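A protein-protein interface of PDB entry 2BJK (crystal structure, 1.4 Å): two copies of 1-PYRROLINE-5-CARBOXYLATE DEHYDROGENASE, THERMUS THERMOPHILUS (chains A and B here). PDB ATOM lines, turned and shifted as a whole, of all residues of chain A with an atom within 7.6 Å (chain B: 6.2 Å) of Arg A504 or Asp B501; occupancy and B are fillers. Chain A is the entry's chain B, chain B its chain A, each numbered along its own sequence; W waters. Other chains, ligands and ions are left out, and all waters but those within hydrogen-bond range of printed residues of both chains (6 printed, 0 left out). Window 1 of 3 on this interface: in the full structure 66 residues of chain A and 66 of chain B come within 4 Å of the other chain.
The side-chain amide oxygen of Asn B494 lies within hydrogen-bond range of the backbone NH of Met A509.
The side-chain carboxylate of Asp B501 sits at hydrogen-bond distance from the side-chain hydroxyl of Tyr A171 (2.6 Å).
The side-chain carboxylate (OD2) of Asp B501 lies within salt-bridge range of the guanidinium group (NE) of Arg A504.
OD2 of Asp A501 lies within salt-bridge range of NE of Arg B504 (2.8 Å).
OH of Tyr B144 is in hydrogen-bond range of N of Leu B500.
The side-chain hydroxyl (OH) of Tyr B152 lies within hydrogen-bond range of the backbone carbonyl oxygen (O) of Leu B500, at 2.6 Å.
The backbone NH of Glu A508 is in hydrogen-bond range of the backbone carbonyl oxygen of Val A172 (2.9 Å).
O of Leu A507 sits at hydrogen-bond distance from NH2 of Arg A504 (2.9 Å).
Leu B500 touches Glu A158 (CD1 to CD, 3.9 Å).
Asn B494 touches Glu A508.
Lys B496 touches Met A509.
Met A509 touches Asp B501.
Arg A504 touches just one residue of chain B: Asp B501 (2.8 Å).
Of chain A, only Tyr A171, Arg A504 and Met A509 come within 4 Å of Asp B501.
Of the printed residues of chain B, Asp A501 touches Arg B504 (2.8 Å).
Of the printed residues of chain B, Glu A158 touches Leu B500 (3.9 Å).
The nearest residue of chain B that does not touch Arg A504 is Asn B494 (4.6 Å).
The nearest printed residue of chain A that does not touch Lys B496 is Lys A510 (4.5 Å).
Hydrophobic or aromatic side chains of chain A that line the printed part of chain B: Tyr A171 and Met A509.
Of the 11 printed residues of chain B, 5 touch a printed residue of chain A.
Hydrophobic or aromatic side chains of chain B within 4 Å of the printed part of chain A: Leu B500.
Among the printed residues, 8 pairs touch across the chains.
Among the printed residues, Asp or Glu carboxylates within 4 Å of a Lys or Arg side-chain nitrogen of the other chain: Asp A501 with Arg B504 and Arg A504 with Asp B501.
Asp A501 touches Arg B504, and with the chains exchanged Arg A504 touches Asp B501.
Positions printed for both chains: 152, 499, 500, 501, 502, 503, 504 and 505.
Of the 8 pairs that touch across the chains among the printed residues, 2 have their exchanged pair printed and touching as well.
Water W5 lies within hydrogen-bond range of the side-chain amide oxygen (OD1) of Asn B494 (2.7 Å), the guanidinium group (NH2) of Arg A504 (3.0 Å), the guanidinium group (NH2) of Arg A284 (3.0 Å) and the backbone carbonyl oxygen (O) of Leu A507 (3.4 Å).
Water W1 bridges OH of Tyr B144 (2.7 Å) and O of Glu A158 (2.8 Å).
Water W6 lies within hydrogen-bond range of OH of Tyr A171 and OD1 of Asp B501.
Water W3 lies within hydrogen-bond range of O of Asn B494, NH1 of Arg A504 and N of Lys B496.
Water W4 lies within hydrogen-bond range of O of Glu A158 (2.8 Å), N of Leu B500 (3.0 Å) and OH of Tyr B144 (3.3 Å).
Water W2 lies within hydrogen-bond range of the side-chain carboxylate (OD1) of Asp B501 (3.1 Å) and the side-chain hydroxyl (OH) of Tyr A171 (3.2 Å).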
ATOM      1  N   TYR A 152      27.172  15.038 -10.439  1.00  0.00           N
ATOM      2  CA  TYR A 152      26.314  16.197 -10.183  1.00  0.00           C
ATOM      3  C   TYR A 152      25.650  16.735 -11.445  1.00  0.00           C
ATOM      4  O   TYR A 152      24.979  17.767 -11.397  1.00  0.00           O
ATOM      5  CB  TYR A 152      27.128  17.341  -9.564  1.00  0.00           C
ATOM      6  CG  TYR A 152      27.686  17.057  -8.192  1.00  0.00           C
ATOM      7  CD1 TYR A 152      28.932  16.454  -8.030  1.00  0.00           C
ATOM      8  CD2 TYR A 152      26.955  17.368  -7.053  1.00  0.00           C
ATOM      9  CE1 TYR A 152      29.434  16.170  -6.766  1.00  0.00           C
ATOM     10  CE2 TYR A 152      27.445  17.086  -5.782  1.00  0.00           C
ATOM     11  CZ  TYR A 152      28.683  16.489  -5.647  1.00  0.00           C
ATOM     12  OH  TYR A 152      29.164  16.224  -4.388  1.00  0.00           O
ATOM     13  N   VAL A 157      19.372  16.035  -8.650  1.00  0.00           N
ATOM     14  CA  VAL A 157      18.715  15.942  -7.350  1.00  0.00           C
ATOM     15  C   VAL A 157      17.515  15.009  -7.258  1.00  0.00           C
ATOM     16  O   VAL A 157      16.620  15.034  -8.097  1.00  0.00           O
ATOM     17  CB  VAL A 157      18.309  17.342  -6.863  1.00  0.00           C
ATOM     18  CG1 VAL A 157      17.738  17.263  -5.455  1.00  0.00           C
ATOM     19  CG2 VAL A 157      19.520  18.268  -6.892  1.00  0.00           C
ATOM     20  N   GLU A 158      17.516  14.183  -6.216  1.00  0.00           N
ATOM     21  CA  GLU A 158      16.438  13.236  -5.954  1.00  0.00           C
ATOM     22  C   GLU A 158      15.287  13.966  -5.253  1.00  0.00           C
ATOM     23  O   GLU A 158      15.435  14.427  -4.116  1.00  0.00           O
ATOM     24  CB  GLU A 158      16.973  12.118  -5.063  1.00  0.00           C
ATOM     25  CG  GLU A 158      16.003  11.004  -4.752  1.00  0.00           C
ATOM     26  CD  GLU A 158      16.592  10.019  -3.761  1.00  0.00           C
ATOM     27  OE1 GLU A 158      17.782   9.670  -3.911  1.00  0.00           O
ATOM     28  OE2 GLU A 158      15.873   9.593  -2.836  1.00  0.00           O
ATOM     29  N   TYR A 171      21.930  21.284 -10.000  1.00  0.00           N
ATOM     30  CA  TYR A 171      22.998  22.141  -9.524  1.00  0.00           C
ATOM     31  C   TYR A 171      23.521  23.086 -10.589  1.00  0.00           C
ATOM     32  O   TYR A 171      23.519  22.772 -11.780  1.00  0.00           O
ATOM     33  CB  TYR A 171      24.154  21.290  -8.995  1.00  0.00           C
ATOM     34  CG  TYR A 171      23.760  20.416  -7.834  1.00  0.00           C
ATOM     35  CD1 TYR A 171      23.649  19.036  -7.978  1.00  0.00           C
ATOM     36  CD2 TYR A 171      23.468  20.975  -6.591  1.00  0.00           C
ATOM     37  CE1 TYR A 171      23.257  18.230  -6.911  1.00  0.00           C
ATOM     38  CE2 TYR A 171      23.073  20.180  -5.519  1.00  0.00           C
ATOM     39  CZ  TYR A 171      22.971  18.809  -5.688  1.00  0.00           C
ATOM     40  OH  TYR A 171      22.584  18.013  -4.634  1.00  0.00           O
ATOM     41  N   VAL A 172      23.956  24.254 -10.137  1.00  0.00           N
ATOM     42  CA  VAL A 172      24.536  25.261 -11.009  1.00  0.00           C
ATOM     43  C   VAL A 172      25.752  25.809 -10.279  1.00  0.00           C
ATOM     44  O   VAL A 172      25.771  25.881  -9.048  1.00  0.00           O
ATOM     45  CB  VAL A 172      23.555  26.419 -11.314  1.00  0.00           C
ATOM     46  CG1 VAL A 172      22.397  25.910 -12.159  1.00  0.00           C
ATOM     47  CG2 VAL A 172      23.050  27.038 -10.032  1.00  0.00           C
ATOM     48  N   LEU A 174      28.665  28.528  -8.940  1.00  0.00           N
ATOM     49  CA  LEU A 174      28.544  29.817  -8.266  1.00  0.00           C
ATOM     50  C   LEU A 174      28.990  31.037  -9.062  1.00  0.00           C
ATOM     51  O   LEU A 174      28.296  32.052  -9.084  1.00  0.00           O
ATOM     52  CB  LEU A 174      29.321  29.782  -6.948  1.00  0.00           C
ATOM     53  CG  LEU A 174      28.987  28.622  -6.009  1.00  0.00           C
ATOM     54  CD1 LEU A 174      29.911  28.665  -4.807  1.00  0.00           C
ATOM     55  CD2 LEU A 174      27.529  28.707  -5.583  1.00  0.00           C
ATOM     56  N   GLY A 196      38.823  21.587  -8.925  1.00  0.00           N
ATOM     57  CA  GLY A 196      37.576  21.130  -8.327  1.00  0.00           C
ATOM     58  C   GLY A 196      36.464  22.112  -8.682  1.00  0.00           C
ATOM     59  O   GLY A 196      35.462  21.725  -9.278  1.00  0.00           O
ATOM     60  N   VAL A 200      33.075  21.845 -12.202  1.00  0.00           N
ATOM     61  CA  VAL A 200      31.624  21.961 -12.197  1.00  0.00           C
ATOM     62  C   VAL A 200      31.064  23.263 -12.755  1.00  0.00           C
ATOM     63  O   VAL A 200      29.874  23.546 -12.612  1.00  0.00           O
ATOM     64  CB  VAL A 200      31.043  21.694 -10.785  1.00  0.00           C
ATOM     65  CG1 VAL A 200      31.331  20.253 -10.375  1.00  0.00           C
ATOM     66  CG2 VAL A 200      31.625  22.669  -9.772  1.00  0.00           C
ATOM     67  N   ARG A 284      31.101  32.422   0.041  1.00  0.00           N
ATOM     68  CA  ARG A 284      31.430  31.127   0.605  1.00  0.00           C
ATOM     69  C   ARG A 284      32.939  31.132   0.744  1.00  0.00           C
ATOM     70  O   ARG A 284      33.651  31.535  -0.177  1.00  0.00           O
ATOM     71  CB  ARG A 284      31.011  29.984  -0.315  1.00  0.00           C
ATOM     72  CG  ARG A 284      29.523  29.813  -0.435  1.00  0.00           C
ATOM     73  CD  ARG A 284      29.190  28.501  -1.111  1.00  0.00           C
ATOM     74  NE  ARG A 284      27.753  28.366  -1.310  1.00  0.00           N
ATOM     75  CZ  ARG A 284      27.174  27.328  -1.901  1.00  0.00           C
ATOM     76  NH1 ARG A 284      27.908  26.323  -2.355  1.00  0.00           N
ATOM     77  NH2 ARG A 284      25.857  27.293  -2.038  1.00  0.00           N
ATOM     78  N   TYR A 286      36.124  28.619   2.098  1.00  0.00           N
ATOM     79  CA  TYR A 286      36.579  27.330   2.582  1.00  0.00           C
ATOM     80  C   TYR A 286      38.025  27.547   2.976  1.00  0.00           C
ATOM     81  O   TYR A 286      38.846  27.960   2.158  1.00  0.00           O
ATOM     82  CB  TYR A 286      36.441  26.273   1.487  1.00  0.00           C
ATOM     83  CG  TYR A 286      35.006  26.140   1.061  1.00  0.00           C
ATOM     84  CD1 TYR A 286      34.579  26.603  -0.179  1.00  0.00           C
ATOM     85  CD2 TYR A 286      34.052  25.625   1.937  1.00  0.00           C
ATOM     86  CE1 TYR A 286      33.238  26.560  -0.539  1.00  0.00           C
ATOM     87  CE2 TYR A 286      32.712  25.579   1.592  1.00  0.00           C
ATOM     88  CZ  TYR A 286      32.310  26.047   0.354  1.00  0.00           C
ATOM     89  OH  TYR A 286      30.984  26.005   0.008  1.00  0.00           O
ATOM     90  N   ALA A 499      37.271  13.972  -2.370  1.00  0.00           N
ATOM     91  CA  ALA A 499      36.037  13.295  -2.007  1.00  0.00           C
ATOM     92  C   ALA A 499      34.892  13.874  -2.823  1.00  0.00           C
ATOM     93  O   ALA A 499      34.940  15.034  -3.242  1.00  0.00           O
ATOM     94  CB  ALA A 499      35.766  13.478  -0.525  1.00  0.00           C
ATOM     95  N   LEU A 500      33.861  13.065  -3.039  1.00  0.00           N
ATOM     96  CA  LEU A 500      32.700  13.491  -3.808  1.00  0.00           C
ATOM     97  C   LEU A 500      32.092  14.770  -3.252  1.00  0.00           C
ATOM     98  O   LEU A 500      31.679  15.651  -4.007  1.00  0.00           O
ATOM     99  CB  LEU A 500      31.643  12.385  -3.812  1.00  0.00           C
ATOM    100  CG  LEU A 500      32.064  11.073  -4.478  1.00  0.00           C
ATOM    101  CD1 LEU A 500      31.033   9.989  -4.198  1.00  0.00           C
ATOM    102  CD2 LEU A 500      32.220  11.296  -5.971  1.00  0.00           C
ATOM    103  N   ASP A 501      32.055  14.869  -1.925  1.00  0.00           N
ATOM    104  CA  ASP A 501      31.481  16.027  -1.238  1.00  0.00           C
ATOM    105  C   ASP A 501      32.164  17.353  -1.546  1.00  0.00           C
ATOM    106  O   ASP A 501      31.546  18.411  -1.435  1.00  0.00           O
ATOM    107  CB  ASP A 501      31.510  15.819   0.283  1.00  0.00           C
ATOM    108  CG  ASP A 501      30.431  14.876   0.775  1.00  0.00           C
ATOM    109  OD1 ASP A 501      29.693  14.303  -0.055  1.00  0.00           O
ATOM    110  OD2 ASP A 501      30.328  14.709   2.008  1.00  0.00           O
ATOM    111  N   TYR A 502      33.431  17.308  -1.937  1.00  0.00           N
ATOM    112  CA  TYR A 502      34.157  18.540  -2.212  1.00  0.00           C
ATOM    113  C   TYR A 502      33.487  19.415  -3.261  1.00  0.00           C
ATOM    114  O   TYR A 502      33.357  20.622  -3.079  1.00  0.00           O
ATOM    115  CB  TYR A 502      35.580  18.222  -2.669  1.00  0.00           C
ATOM    116  CG  TYR A 502      36.520  19.407  -2.693  1.00  0.00           C
ATOM    117  CD1 TYR A 502      36.885  20.053  -1.511  1.00  0.00           C
ATOM    118  CD2 TYR A 502      37.115  19.825  -3.882  1.00  0.00           C
ATOM    119  CE1 TYR A 502      37.832  21.078  -1.513  1.00  0.00           C
ATOM    120  CE2 TYR A 502      38.063  20.846  -3.894  1.00  0.00           C
ATOM    121  CZ  TYR A 502      38.419  21.461  -2.707  1.00  0.00           C
ATOM    122  OH  TYR A 502      39.403  22.421  -2.715  1.00  0.00           O
ATOM    123  N   LEU A 503      33.043  18.804  -4.351  1.00  0.00           N
ATOM    124  CA  LEU A 503      32.453  19.577  -5.431  1.00  0.00           C
ATOM    125  C   LEU A 503      31.137  20.256  -5.083  1.00  0.00           C
ATOM    126  O   LEU A 503      30.811  21.304  -5.639  1.00  0.00           O
ATOM    127  CB  LEU A 503      32.296  18.700  -6.674  1.00  0.00           C
ATOM    128  CG  LEU A 503      33.600  18.044  -7.156  1.00  0.00           C
ATOM    129  CD1 LEU A 503      33.322  17.297  -8.450  1.00  0.00           C
ATOM    130  CD2 LEU A 503      34.702  19.086  -7.369  1.00  0.00           C
ATOM    131  N   ARG A 504      30.391  19.671  -4.153  1.00  0.00           N
ATOM    132  CA  ARG A 504      29.118  20.240  -3.730  1.00  0.00           C
ATOM    133  C   ARG A 504      29.310  21.642  -3.151  1.00  0.00           C
ATOM    134  O   ARG A 504      28.412  22.487  -3.213  1.00  0.00           O
ATOM    135  CB  ARG A 504      28.471  19.343  -2.673  1.00  0.00           C
ATOM    136  CG  ARG A 504      27.137  19.863  -2.148  1.00  0.00           C
ATOM    137  CD  ARG A 504      26.094  19.878  -3.249  1.00  0.00           C
ATOM    138  NE  ARG A 504      24.796  20.372  -2.798  1.00  0.00           N
ATOM    139  CZ  ARG A 504      24.475  21.654  -2.665  1.00  0.00           C
ATOM    140  NH1 ARG A 504      23.258  21.983  -2.247  1.00  0.00           N
ATOM    141  NH2 ARG A 504      25.355  22.608  -2.952  1.00  0.00           N
ATOM    142  N   LEU A 505      30.488  21.877  -2.582  1.00  0.00           N
ATOM    143  CA  LEU A 505      30.804  23.168  -1.980  1.00  0.00           C
ATOM    144  C   LEU A 505      30.825  24.301  -2.993  1.00  0.00           C
ATOM    145  O   LEU A 505      30.681  25.469  -2.631  1.00  0.00           O
ATOM    146  CB  LEU A 505      32.171  23.104  -1.296  1.00  0.00           C
ATOM    147  CG  LEU A 505      32.317  22.062  -0.190  1.00  0.00           C
ATOM    148  CD1 LEU A 505      33.757  22.051   0.292  1.00  0.00           C
ATOM    149  CD2 LEU A 505      31.355  22.374   0.952  1.00  0.00           C
ATOM    150  N   PHE A 506      30.993  23.958  -4.266  1.00  0.00           N
ATOM    151  CA  PHE A 506      31.076  24.967  -5.311  1.00  0.00           C
ATOM    152  C   PHE A 506      29.868  24.997  -6.233  1.00  0.00           C
ATOM    153  O   PHE A 506      29.944  25.443  -7.383  1.00  0.00           O
ATOM    154  CB  PHE A 506      32.374  24.755  -6.090  1.00  0.00           C
ATOM    155  CG  PHE A 506      33.586  24.732  -5.190  1.00  0.00           C
ATOM    156  CD1 PHE A 506      34.083  23.529  -4.697  1.00  0.00           C
ATOM    157  CD2 PHE A 506      34.160  25.919  -4.746  1.00  0.00           C
ATOM    158  CE1 PHE A 506      35.129  23.512  -3.772  1.00  0.00           C
ATOM    159  CE2 PHE A 506      35.205  25.911  -3.821  1.00  0.00           C
ATOM    160  CZ  PHE A 506      35.688  24.707  -3.333  1.00  0.00           C
ATOM    161  N   LEU A 507      28.740  24.546  -5.693  1.00  0.00           N
ATOM    162  CA  LEU A 507      27.482  24.508  -6.424  1.00  0.00           C
ATOM    163  C   LEU A 507      26.332  25.011  -5.565  1.00  0.00           C
ATOM    164  O   LEU A 507      26.394  24.967  -4.335  1.00  0.00           O
ATOM    165  CB  LEU A 507      27.151  23.068  -6.835  1.00  0.00           C
ATOM    166  CG  LEU A 507      28.098  22.360  -7.799  1.00  0.00           C
ATOM    167  CD1 LEU A 507      27.783  20.868  -7.819  1.00  0.00           C
ATOM    168  CD2 LEU A 507      27.960  22.972  -9.180  1.00  0.00           C
ATOM    169  N   GLU A 508      25.294  25.506  -6.227  1.00  0.00           N
ATOM    170  CA  GLU A 508      24.077  25.910  -5.541  1.00  0.00           C
ATOM    171  C   GLU A 508      22.971  25.145  -6.261  1.00  0.00           C
ATOM    172  O   GLU A 508      23.167  24.675  -7.385  1.00  0.00           O
ATOM    173  CB  GLU A 508      23.859  27.434  -5.563  1.00  0.00           C
ATOM    174  CG  GLU A 508      24.003  28.146  -6.885  1.00  0.00           C
ATOM    175  CD  GLU A 508      24.076  29.660  -6.706  1.00  0.00           C
ATOM    176  OE1 GLU A 508      24.036  30.130  -5.547  1.00  0.00           O
ATOM    177  OE2 GLU A 508      24.178  30.379  -7.720  1.00  0.00           O
ATOM    178  N   MET A 509      21.826  24.984  -5.612  1.00  0.00           N
ATOM    179  CA  MET A 509      20.735  24.216  -6.198  1.00  0.00           C
ATOM    180  C   MET A 509      19.535  25.052  -6.600  1.00  0.00           C
ATOM    181  O   MET A 509      19.142  25.985  -5.895  1.00  0.00           O
ATOM    182  CB  MET A 509      20.278  23.133  -5.216  1.00  0.00           C
ATOM    183  CG  MET A 509      19.313  22.119  -5.823  1.00  0.00           C
ATOM    184  SD  MET A 509      18.361  21.179  -4.597  1.00  0.00           S
ATOM    185  CE  MET A 509      19.675  20.318  -3.699  1.00  0.00           C
ATOM    186  N   LYS A 510      18.958  24.693  -7.741  1.00  0.00           N
ATOM    187  CA  LYS A 510      17.775  25.356  -8.272  1.00  0.00           C
ATOM    188  C   LYS A 510      16.675  24.302  -8.398  1.00  0.00           C
ATOM    189  O   LYS A 510      16.942  23.172  -8.811  1.00  0.00           O
ATOM    190  CB  LYS A 510      18.076  25.949  -9.651  1.00  0.00           C
ATOM    191  CG  LYS A 510      16.997  26.868 -10.192  1.00  0.00           C
ATOM    192  CD  LYS A 510      17.477  27.533 -11.470  1.00  0.00           C
ATOM    193  CE  LYS A 510      16.503  28.584 -11.960  1.00  0.00           C
ATOM    194  NZ  LYS A 510      17.018  29.253 -13.192  1.00  0.00           N
ATOM    195  N   TYR B 144      10.107  13.848   6.648  1.00  0.00           N
ATOM    196  CA  TYR B 144      11.142  13.845   5.627  1.00  0.00           C
ATOM    197  C   TYR B 144      12.540  13.724   6.216  1.00  0.00           C
ATOM    198  O   TYR B 144      13.320  12.867   5.798  1.00  0.00           O
ATOM    199  CB  TYR B 144      11.042  15.117   4.776  1.00  0.00           C
ATOM    200  CG  TYR B 144      11.965  15.123   3.581  1.00  0.00           C
ATOM    201  CD1 TYR B 144      11.552  14.609   2.349  1.00  0.00           C
ATOM    202  CD2 TYR B 144      13.269  15.592   3.695  1.00  0.00           C
ATOM    203  CE1 TYR B 144      12.429  14.565   1.258  1.00  0.00           C
ATOM    204  CE2 TYR B 144      14.146  15.550   2.620  1.00  0.00           C
ATOM    205  CZ  TYR B 144      13.724  15.038   1.410  1.00  0.00           C
ATOM    206  OH  TYR B 144      14.603  15.001   0.351  1.00  0.00           O
ATOM    207  N   TYR B 152      22.539   9.067   5.757  1.00  0.00           N
ATOM    208  CA  TYR B 152      23.868   9.480   6.209  1.00  0.00           C
ATOM    209  C   TYR B 152      24.428   8.575   7.300  1.00  0.00           C
ATOM    210  O   TYR B 152      25.490   8.855   7.855  1.00  0.00           O
ATOM    211  CB  TYR B 152      23.826  10.912   6.761  1.00  0.00           C
ATOM    212  CG  TYR B 152      23.514  11.978   5.739  1.00  0.00           C
ATOM    213  CD1 TYR B 152      22.197  12.332   5.444  1.00  0.00           C
ATOM    214  CD2 TYR B 152      24.539  12.628   5.056  1.00  0.00           C
ATOM    215  CE1 TYR B 152      21.910  13.306   4.493  1.00  0.00           C
ATOM    216  CE2 TYR B 152      24.265  13.604   4.103  1.00  0.00           C
ATOM    217  CZ  TYR B 152      22.951  13.937   3.828  1.00  0.00           C
ATOM    218  OH  TYR B 152      22.686  14.907   2.888  1.00  0.00           O
ATOM    219  N   ASN B 494      21.512  29.458   0.440  1.00  0.00           N
ATOM    220  CA  ASN B 494      21.031  28.330  -0.356  1.00  0.00           C
ATOM    221  C   ASN B 494      20.972  27.010   0.406  1.00  0.00           C
ATOM    222  O   ASN B 494      21.281  25.954  -0.144  1.00  0.00           O
ATOM    223  CB  ASN B 494      21.888  28.164  -1.628  1.00  0.00           C
ATOM    224  CG  ASN B 494      21.213  27.298  -2.688  1.00  0.00           C
ATOM    225  OD1 ASN B 494      21.755  26.272  -3.106  1.00  0.00           O
ATOM    226  ND2 ASN B 494      20.035  27.715  -3.133  1.00  0.00           N
ATOM    227  N   LYS B 496      19.023  24.359   1.200  1.00  0.00           N
ATOM    228  CA  LYS B 496      17.763  23.829   0.693  1.00  0.00           C
ATOM    229  C   LYS B 496      16.989  22.991   1.698  1.00  0.00           C
ATOM    230  O   LYS B 496      17.344  21.846   1.975  1.00  0.00           O
ATOM    231  CB  LYS B 496      18.020  23.011  -0.575  1.00  0.00           C
ATOM    232  CG  LYS B 496      18.344  23.851  -1.809  1.00  0.00           C
ATOM    233  CD  LYS B 496      17.177  24.763  -2.168  1.00  0.00           C
ATOM    234  CE  LYS B 496      17.112  25.042  -3.659  1.00  0.00           C
ATOM    235  NZ  LYS B 496      15.940  25.890  -4.000  1.00  0.00           N
ATOM    236  N   ALA B 499      15.089  18.836   1.633  1.00  0.00           N
ATOM    237  CA  ALA B 499      15.912  18.156   0.646  1.00  0.00           C
ATOM    238  C   ALA B 499      16.987  17.361   1.366  1.00  0.00           C
ATOM    239  O   ALA B 499      17.393  17.718   2.475  1.00  0.00           O
ATOM    240  CB  ALA B 499      16.556  19.173  -0.285  1.00  0.00           C
ATOM    241  N   LEU B 500      17.453  16.294   0.726  1.00  0.00           N
ATOM    242  CA  LEU B 500      18.489  15.447   1.304  1.00  0.00           C
ATOM    243  C   LEU B 500      19.725  16.256   1.690  1.00  0.00           C
ATOM    244  O   LEU B 500      20.329  16.018   2.735  1.00  0.00           O
ATOM    245  CB  LEU B 500      18.883  14.352   0.308  1.00  0.00           C
ATOM    246  CG  LEU B 500      17.755  13.399  -0.100  1.00  0.00           C
ATOM    247  CD1 LEU B 500      18.208  12.498  -1.234  1.00  0.00           C
ATOM    248  CD2 LEU B 500      17.333  12.578   1.103  1.00  0.00           C
ATOM    249  N   ASP B 501      20.086  17.222   0.847  1.00  0.00           N
ATOM    250  CA  ASP B 501      21.261  18.057   1.074  1.00  0.00           C
ATOM    251  C   ASP B 501      21.227  18.867   2.361  1.00  0.00           C
ATOM    252  O   ASP B 501      22.273  19.223   2.895  1.00  0.00           O
ATOM    253  CB  ASP B 501      21.460  19.027  -0.096  1.00  0.00           C
ATOM    254  CG  ASP B 501      22.056  18.368  -1.324  1.00  0.00           C
ATOM    255  OD1 ASP B 501      22.269  17.135  -1.324  1.00  0.00           O
ATOM    256  OD2 ASP B 501      22.311  19.103  -2.305  1.00  0.00           O
ATOM    257  N   TYR B 502      20.034  19.163   2.864  1.00  0.00           N
ATOM    258  CA  TYR B 502      19.921  19.964   4.075  1.00  0.00           C
ATOM    259  C   TYR B 502      20.682  19.383   5.256  1.00  0.00           C
ATOM    260  O   TYR B 502      21.397  20.099   5.956  1.00  0.00           O
ATOM    261  CB  TYR B 502      18.453  20.125   4.468  1.00  0.00           C
ATOM    262  CG  TYR B 502      18.197  21.192   5.512  1.00  0.00           C
ATOM    263  CD1 TYR B 502      18.434  22.540   5.231  1.00  0.00           C
ATOM    264  CD2 TYR B 502      17.638  20.868   6.748  1.00  0.00           C
ATOM    265  CE1 TYR B 502      18.109  23.540   6.154  1.00  0.00           C
ATOM    266  CE2 TYR B 502      17.310  21.859   7.673  1.00  0.00           C
ATOM    267  CZ  TYR B 502      17.541  23.188   7.366  1.00  0.00           C
ATOM    268  OH  TYR B 502      17.155  24.164   8.256  1.00  0.00           O
ATOM    269  N   LEU B 503      20.550  18.082   5.474  1.00  0.00           N
ATOM    270  CA  LEU B 503      21.197  17.474   6.627  1.00  0.00           C
ATOM    271  C   LEU B 503      22.720  17.478   6.589  1.00  0.00           C
ATOM    272  O   LEU B 503      23.372  17.514   7.635  1.00  0.00           O
ATOM    273  CB  LEU B 503      20.662  16.054   6.835  1.00  0.00           C
ATOM    274  CG  LEU B 503      19.134  15.962   6.973  1.00  0.00           C
ATOM    275  CD1 LEU B 503      18.750  14.524   7.283  1.00  0.00           C
ATOM    276  CD2 LEU B 503      18.626  16.894   8.071  1.00  0.00           C
ATOM    277  N   ARG B 504      23.286  17.458   5.389  1.00  0.00           N
ATOM    278  CA  ARG B 504      24.737  17.465   5.240  1.00  0.00           C
ATOM    279  C   ARG B 504      25.346  18.723   5.865  1.00  0.00           C
ATOM    280  O   ARG B 504      26.504  18.720   6.295  1.00  0.00           O
ATOM    281  CB  ARG B 504      25.101  17.402   3.754  1.00  0.00           C
ATOM    282  CG  ARG B 504      26.594  17.429   3.467  1.00  0.00           C
ATOM    283  CD  ARG B 504      27.263  16.194   4.018  1.00  0.00           C
ATOM    284  NE  ARG B 504      28.706  16.187   3.795  1.00  0.00           N
ATOM    285  CZ  ARG B 504      29.590  16.851   4.534  1.00  0.00           C
ATOM    286  NH1 ARG B 504      30.882  16.768   4.238  1.00  0.00           N
ATOM    287  NH2 ARG B 504      29.192  17.590   5.565  1.00  0.00           N
ATOM    288  N   LEU B 505      24.557  19.793   5.905  1.00  0.00           N
ATOM    289  CA  LEU B 505      25.004  21.068   6.457  1.00  0.00           C
ATOM    290  C   LEU B 505      25.308  20.989   7.945  1.00  0.00           C
ATOM    291  O   LEU B 505      26.065  21.801   8.481  1.00  0.00           O
ATOM    292  CB  LEU B 505      23.933  22.134   6.233  1.00  0.00           C
ATOM    293  CG  LEU B 505      23.550  22.399   4.777  1.00  0.00           C
ATOM    294  CD1 LEU B 505      22.375  23.361   4.735  1.00  0.00           C
ATOM    295  CD2 LEU B 505      24.741  22.957   4.019  1.00  0.00           C
HETATM  296  O   HOH W   1      13.783  13.748  -1.928  1.00  0.00           O
HETATM  297  O   HOH W   2      24.971  16.772  -2.841  1.00  0.00           O
HETATM  298  O   HOH W   3      21.518  23.160  -0.059  1.00  0.00           O
HETATM  299  O   HOH W   4      16.458  16.182  -2.136  1.00  0.00           O
HETATM  300  O   HOH W   5      23.912  25.033  -2.019  1.00  0.00           O
HETATM  301  O   HOH W   6      20.994  15.973  -3.574  1.00  0.00           O
